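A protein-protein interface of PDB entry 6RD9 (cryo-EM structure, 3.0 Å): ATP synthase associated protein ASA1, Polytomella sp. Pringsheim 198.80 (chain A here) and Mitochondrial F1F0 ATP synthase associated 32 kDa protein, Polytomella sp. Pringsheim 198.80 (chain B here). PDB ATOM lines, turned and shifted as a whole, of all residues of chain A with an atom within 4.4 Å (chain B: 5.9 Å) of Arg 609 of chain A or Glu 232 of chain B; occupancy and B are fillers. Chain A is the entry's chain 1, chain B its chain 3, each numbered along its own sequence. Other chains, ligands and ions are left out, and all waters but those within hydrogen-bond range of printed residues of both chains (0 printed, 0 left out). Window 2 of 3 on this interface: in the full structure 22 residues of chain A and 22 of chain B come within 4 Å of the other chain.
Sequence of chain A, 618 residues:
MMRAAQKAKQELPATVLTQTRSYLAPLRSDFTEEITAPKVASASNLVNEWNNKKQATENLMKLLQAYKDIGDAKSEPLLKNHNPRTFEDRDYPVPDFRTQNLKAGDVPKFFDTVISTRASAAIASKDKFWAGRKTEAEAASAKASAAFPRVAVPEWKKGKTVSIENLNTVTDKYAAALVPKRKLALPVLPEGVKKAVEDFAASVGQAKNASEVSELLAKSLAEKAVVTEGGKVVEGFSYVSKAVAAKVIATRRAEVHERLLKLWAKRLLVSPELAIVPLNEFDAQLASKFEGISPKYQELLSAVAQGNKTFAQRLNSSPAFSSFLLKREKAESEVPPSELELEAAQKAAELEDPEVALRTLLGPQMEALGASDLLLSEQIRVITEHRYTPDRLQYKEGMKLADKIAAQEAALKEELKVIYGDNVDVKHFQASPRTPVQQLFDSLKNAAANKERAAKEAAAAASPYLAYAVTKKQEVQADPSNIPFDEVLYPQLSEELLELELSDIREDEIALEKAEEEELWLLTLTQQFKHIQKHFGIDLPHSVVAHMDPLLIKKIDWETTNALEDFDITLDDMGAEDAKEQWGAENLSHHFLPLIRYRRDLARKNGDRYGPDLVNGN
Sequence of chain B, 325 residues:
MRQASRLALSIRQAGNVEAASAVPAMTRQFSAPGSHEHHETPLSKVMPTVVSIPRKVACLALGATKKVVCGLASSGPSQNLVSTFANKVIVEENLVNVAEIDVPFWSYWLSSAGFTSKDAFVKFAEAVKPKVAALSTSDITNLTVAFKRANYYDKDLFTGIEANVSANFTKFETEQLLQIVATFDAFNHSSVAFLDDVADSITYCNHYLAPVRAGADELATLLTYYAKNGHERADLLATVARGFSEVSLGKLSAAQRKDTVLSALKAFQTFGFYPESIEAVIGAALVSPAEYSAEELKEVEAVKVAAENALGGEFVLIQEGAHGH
Glu 232 of chain B touches Leu 614 of chain A.
Ala 234 of chain B touches Leu 614 of chain A (CB to C, 3.6 Å).
Ala 234 of chain B touches Val 615 of chain A.
Phe 271 of chain B touches Val 615 of chain A.
Arg 609 of chain A touches one residue of chain B.
Of chain A, only Arg 609, Asp 613, Leu 614 and Val 615 come within 4 Å of Glu 232 of chain B.
Of the printed residues of chain B, Asp 613 of chain A touches Glu 232 (3.2 Å), Arg 233 (3.4 Å) and Ala 234 (2.5 Å).
Of the printed residues of chain A, Arg 233 of chain B touches Asp 613 (3.4 Å).
Of the printed residues of chain A, Ala 234 of chain B touches Asp 613, Leu 614 and Val 615.
Gly 607 of chain A touches none of the printed residues of chain B.
The side-chain carboxylate (OE1) of Glu 232 of chain B is in salt-bridge range of the guanidinium group (NH1) of Arg 609 of chain A.
The backbone carbonyl oxygen (O) of Asp 613 of chain A sits close to the backbone carbonyl oxygen (O) of Glu 232 of chain B, 3.2 Å away.
O of Asp 613 of chain A is in hydrogen-bond range of N of Ala 234 of chain B.
The side-chain carboxylate (OD1) of Asp 613 of chain A lies within salt-bridge range of the guanidinium group (NE) of Arg 233 of chain B, at 3.8 Å.
The side-chain carboxylate (OE2) of Glu 232 of chain B lies within hydrogen-bond range of the backbone NH (N) of Val 615 of chain A, 2.6 Å away.
Of the 9 printed residues of chain A, 4 touch a printed residue of chain B.
Printed residues of chain A that touch a printed residue of chain B: Arg 609, Asp 613, Leu 614 and Val 615.
Along chain A the printed residues that touch a printed residue of chain B span positions 609 to 615.
Printed residues of chain B that touch a printed residue of chain A: Glu 232, Arg 233, Ala 234 and Phe 271.
Hydrophobic or aromatic side chains of chain B that line the printed part of chain A: Ala 234.
Among the printed residues, 9 pairs touch across the chains.
Among the printed residues, Asp or Glu carboxylates within 4 Å of a Lys or Arg side-chain nitrogen of the other chain: Arg 609 of chain A with Glu 232 of chain B and Asp 613 of chain A with Arg 233 of chain B.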
ATOM      1  N   ALA A 603      19.305  18.651 -15.835  1.00  0.00           N
ATOM      2  CA  ALA A 603      18.687  18.728 -17.145  1.00  0.00           C
ATOM      3  C   ALA A 603      18.038  17.426 -17.567  1.00  0.00           C
ATOM      4  O   ALA A 603      17.151  17.449 -18.416  1.00  0.00           O
ATOM      5  CB  ALA A 603      19.719  19.147 -18.180  1.00  0.00           C
ATOM      6  N   GLY A 607      13.840  17.192 -18.214  1.00  0.00           N
ATOM      7  CA  GLY A 607      13.480  16.813 -19.556  1.00  0.00           C
ATOM      8  C   GLY A 607      14.445  17.218 -20.645  1.00  0.00           C
ATOM      9  O   GLY A 607      14.375  16.663 -21.742  1.00  0.00           O
ATOM     10  N   ASP A 608      15.348  18.151 -20.387  1.00  0.00           N
ATOM     11  CA  ASP A 608      16.210  18.679 -21.429  1.00  0.00           C
ATOM     12  C   ASP A 608      17.410  17.763 -21.636  1.00  0.00           C
ATOM     13  O   ASP A 608      17.479  16.648 -21.116  1.00  0.00           O
ATOM     14  CB  ASP A 608      16.654  20.095 -21.082  1.00  0.00           C
ATOM     15  CG  ASP A 608      15.493  21.007 -20.784  1.00  0.00           C
ATOM     16  OD1 ASP A 608      14.447  20.871 -21.447  1.00  0.00           O
ATOM     17  OD2 ASP A 608      15.620  21.853 -19.880  1.00  0.00           O
ATOM     18  N   ARG A 609      18.359  18.220 -22.431  1.00  0.00           N
ATOM     19  CA  ARG A 609      19.630  17.546 -22.592  1.00  0.00           C
ATOM     20  C   ARG A 609      20.709  18.439 -22.016  1.00  0.00           C
ATOM     21  O   ARG A 609      20.564  19.663 -21.987  1.00  0.00           O
ATOM     22  CB  ARG A 609      19.932  17.250 -24.055  1.00  0.00           C
ATOM     23  CG  ARG A 609      18.925  16.359 -24.723  1.00  0.00           C
ATOM     24  CD  ARG A 609      19.082  16.445 -26.214  1.00  0.00           C
ATOM     25  NE  ARG A 609      19.728  15.271 -26.777  1.00  0.00           N
ATOM     26  CZ  ARG A 609      20.310  15.249 -27.969  1.00  0.00           C
ATOM     27  NH1 ARG A 609      20.871  14.139 -28.415  1.00  0.00           N
ATOM     28  NH2 ARG A 609      20.346  16.344 -28.711  1.00  0.00           N
ATOM     29  N   TYR A 610      21.786  17.827 -21.543  1.00  0.00           N
ATOM     30  CA  TYR A 610      22.909  18.629 -21.096  1.00  0.00           C
ATOM     31  C   TYR A 610      23.597  19.227 -22.308  1.00  0.00           C
ATOM     32  O   TYR A 610      23.819  18.543 -23.306  1.00  0.00           O
ATOM     33  CB  TYR A 610      23.883  17.800 -20.275  1.00  0.00           C
ATOM     34  CG  TYR A 610      24.867  18.654 -19.535  1.00  0.00           C
ATOM     35  CD1 TYR A 610      24.491  19.878 -19.026  1.00  0.00           C
ATOM     36  CD2 TYR A 610      26.173  18.248 -19.360  1.00  0.00           C
ATOM     37  CE1 TYR A 610      25.378  20.668 -18.365  1.00  0.00           C
ATOM     38  CE2 TYR A 610      27.072  19.040 -18.699  1.00  0.00           C
ATOM     39  CZ  TYR A 610      26.666  20.244 -18.200  1.00  0.00           C
ATOM     40  OH  TYR A 610      27.560  21.041 -17.534  1.00  0.00           O
ATOM     41  N   GLY A 611      23.905  20.511 -22.218  1.00  0.00           N
ATOM     42  CA  GLY A 611      24.500  21.271 -23.288  1.00  0.00           C
ATOM     43  C   GLY A 611      25.816  20.748 -23.820  1.00  0.00           C
ATOM     44  O   GLY A 611      25.922  20.406 -24.997  1.00  0.00           O
ATOM     45  N   ASP A 613      27.277  17.953 -23.511  1.00  0.00           N
ATOM     46  CA  ASP A 613      27.330  16.566 -23.947  1.00  0.00           C
ATOM     47  C   ASP A 613      27.118  16.429 -25.441  1.00  0.00           C
ATOM     48  O   ASP A 613      27.488  15.402 -26.009  1.00  0.00           O
ATOM     49  CB  ASP A 613      26.270  15.731 -23.235  1.00  0.00           C
ATOM     50  CG  ASP A 613      26.652  15.376 -21.826  1.00  0.00           C
ATOM     51  OD1 ASP A 613      27.745  15.767 -21.385  1.00  0.00           O
ATOM     52  OD2 ASP A 613      25.852  14.702 -21.153  1.00  0.00           O
ATOM     53  N   LEU A 614      26.526  17.424 -26.083  1.00  0.00           N
ATOM     54  CA  LEU A 614      26.111  17.347 -27.473  1.00  0.00           C
ATOM     55  C   LEU A 614      27.170  17.951 -28.374  1.00  0.00           C
ATOM     56  O   LEU A 614      27.942  18.817 -27.966  1.00  0.00           O
ATOM     57  CB  LEU A 614      24.792  18.083 -27.682  1.00  0.00           C
ATOM     58  CG  LEU A 614      23.766  17.905 -26.577  1.00  0.00           C
ATOM     59  CD1 LEU A 614      22.615  18.831 -26.812  1.00  0.00           C
ATOM     60  CD2 LEU A 614      23.298  16.473 -26.516  1.00  0.00           C
ATOM     61  N   VAL A 615      27.186  17.491 -29.623  1.00  0.00           N
ATOM     62  CA  VAL A 615      28.190  17.957 -30.571  1.00  0.00           C
ATOM     63  C   VAL A 615      27.905  19.393 -30.983  1.00  0.00           C
ATOM     64  O   VAL A 615      28.725  20.294 -30.781  1.00  0.00           O
ATOM     65  CB  VAL A 615      28.246  17.030 -31.791  1.00  0.00           C
ATOM     66  CG1 VAL A 615      29.217  17.573 -32.787  1.00  0.00           C
ATOM     67  CG2 VAL A 615      28.652  15.652 -31.371  1.00  0.00           C
ATOM     68  N   TYR B 226      27.724   3.221 -28.345  1.00  0.00           N
ATOM     69  CA  TYR B 226      27.107   4.500 -28.069  1.00  0.00           C
ATOM     70  C   TYR B 226      26.255   4.987 -29.220  1.00  0.00           C
ATOM     71  O   TYR B 226      25.432   5.880 -29.021  1.00  0.00           O
ATOM     72  CB  TYR B 226      28.171   5.545 -27.715  1.00  0.00           C
ATOM     73  CG  TYR B 226      28.510   5.501 -26.250  1.00  0.00           C
ATOM     74  CD1 TYR B 226      28.087   6.488 -25.387  1.00  0.00           C
ATOM     75  CD2 TYR B 226      29.211   4.436 -25.726  1.00  0.00           C
ATOM     76  CE1 TYR B 226      28.367   6.417 -24.061  1.00  0.00           C
ATOM     77  CE2 TYR B 226      29.494   4.363 -24.405  1.00  0.00           C
ATOM     78  CZ  TYR B 226      29.072   5.351 -23.582  1.00  0.00           C
ATOM     79  OH  TYR B 226      29.361   5.270 -22.256  1.00  0.00           O
ATOM     80  N   GLY B 230      22.097   5.222 -29.154  1.00  0.00           N
ATOM     81  CA  GLY B 230      21.691   6.584 -29.442  1.00  0.00           C
ATOM     82  C   GLY B 230      22.186   7.609 -28.456  1.00  0.00           C
ATOM     83  O   GLY B 230      21.542   8.644 -28.271  1.00  0.00           O
ATOM     84  N   HIS B 231      23.316   7.348 -27.816  1.00  0.00           N
ATOM     85  CA  HIS B 231      23.814   8.147 -26.708  1.00  0.00           C
ATOM     86  C   HIS B 231      24.888   9.077 -27.232  1.00  0.00           C
ATOM     87  O   HIS B 231      25.969   8.628 -27.607  1.00  0.00           O
ATOM     88  CB  HIS B 231      24.362   7.238 -25.619  1.00  0.00           C
ATOM     89  CG  HIS B 231      24.187   7.781 -24.245  1.00  0.00           C
ATOM     90  ND1 HIS B 231      24.877   8.877 -23.789  1.00  0.00           N
ATOM     91  CD2 HIS B 231      23.400   7.381 -23.222  1.00  0.00           C
ATOM     92  CE1 HIS B 231      24.522   9.131 -22.546  1.00  0.00           C
ATOM     93  NE2 HIS B 231      23.629   8.235 -22.176  1.00  0.00           N
ATOM     94  N   GLU B 232      24.595  10.364 -27.274  1.00  0.00           N
ATOM     95  CA  GLU B 232      25.546  11.341 -27.779  1.00  0.00           C
ATOM     96  C   GLU B 232      26.258  11.973 -26.598  1.00  0.00           C
ATOM     97  O   GLU B 232      25.669  12.769 -25.862  1.00  0.00           O
ATOM     98  CB  GLU B 232      24.849  12.396 -28.623  1.00  0.00           C
ATOM     99  CG  GLU B 232      25.787  13.416 -29.211  1.00  0.00           C
ATOM    100  CD  GLU B 232      25.063  14.443 -30.056  1.00  0.00           C
ATOM    101  OE1 GLU B 232      23.953  14.146 -30.544  1.00  0.00           O
ATOM    102  OE2 GLU B 232      25.596  15.552 -30.224  1.00  0.00           O
ATOM    103  N   ARG B 233      27.524  11.605 -26.413  1.00  0.00           N
ATOM    104  CA  ARG B 233      28.412  12.180 -25.408  1.00  0.00           C
ATOM    105  C   ARG B 233      29.559  12.748 -26.213  1.00  0.00           C
ATOM    106  O   ARG B 233      30.468  12.006 -26.557  1.00  0.00           O
ATOM    107  CB  ARG B 233      28.895  11.134 -24.433  1.00  0.00           C
ATOM    108  CG  ARG B 233      27.859  10.597 -23.500  1.00  0.00           C
ATOM    109  CD  ARG B 233      27.549  11.599 -22.445  1.00  0.00           C
ATOM    110  NE  ARG B 233      28.764  12.187 -21.926  1.00  0.00           N
ATOM    111  CZ  ARG B 233      29.315  11.843 -20.779  1.00  0.00           C
ATOM    112  NH1 ARG B 233      30.423  12.430 -20.379  1.00  0.00           N
ATOM    113  NH2 ARG B 233      28.745  10.924 -20.033  1.00  0.00           N
ATOM    114  N   ALA B 234      29.528  14.039 -26.523  1.00  0.00           N
ATOM    115  CA  ALA B 234      30.550  14.596 -27.398  1.00  0.00           C
ATOM    116  C   ALA B 234      31.895  14.724 -26.718  1.00  0.00           C
ATOM    117  O   ALA B 234      32.896  14.951 -27.397  1.00  0.00           O
ATOM    118  CB  ALA B 234      30.133  15.961 -27.915  1.00  0.00           C
ATOM    119  N   LEU B 237      33.479  11.211 -27.301  1.00  0.00           N
ATOM    120  CA  LEU B 237      33.896  10.974 -28.670  1.00  0.00           C
ATOM    121  C   LEU B 237      35.200  11.670 -28.993  1.00  0.00           C
ATOM    122  O   LEU B 237      35.922  11.220 -29.875  1.00  0.00           O
ATOM    123  CB  LEU B 237      32.827  11.442 -29.640  1.00  0.00           C
ATOM    124  CG  LEU B 237      31.424  10.904 -29.454  1.00  0.00           C
ATOM    125  CD1 LEU B 237      30.514  11.582 -30.429  1.00  0.00           C
ATOM    126  CD2 LEU B 237      31.402   9.417 -29.617  1.00  0.00           C
ATOM    127  N   PHE B 271      26.671  10.478 -34.960  1.00  0.00           N
ATOM    128  CA  PHE B 271      26.650  11.675 -34.143  1.00  0.00           C
ATOM    129  C   PHE B 271      27.019  12.919 -34.918  1.00  0.00           C
ATOM    130  O   PHE B 271      26.792  14.022 -34.423  1.00  0.00           O
ATOM    131  CB  PHE B 271      27.601  11.519 -32.968  1.00  0.00           C
ATOM    132  CG  PHE B 271      27.388  10.270 -32.214  1.00  0.00           C
ATOM    133  CD1 PHE B 271      26.233  10.083 -31.490  1.00  0.00           C
ATOM    134  CD2 PHE B 271      28.328   9.277 -32.244  1.00  0.00           C
ATOM    135  CE1 PHE B 271      26.030   8.932 -30.807  1.00  0.00           C
ATOM    136  CE2 PHE B 271      28.131   8.121 -31.571  1.00  0.00           C
ATOM    137  CZ  PHE B 271      26.985   7.952 -30.843  1.00  0.00           C
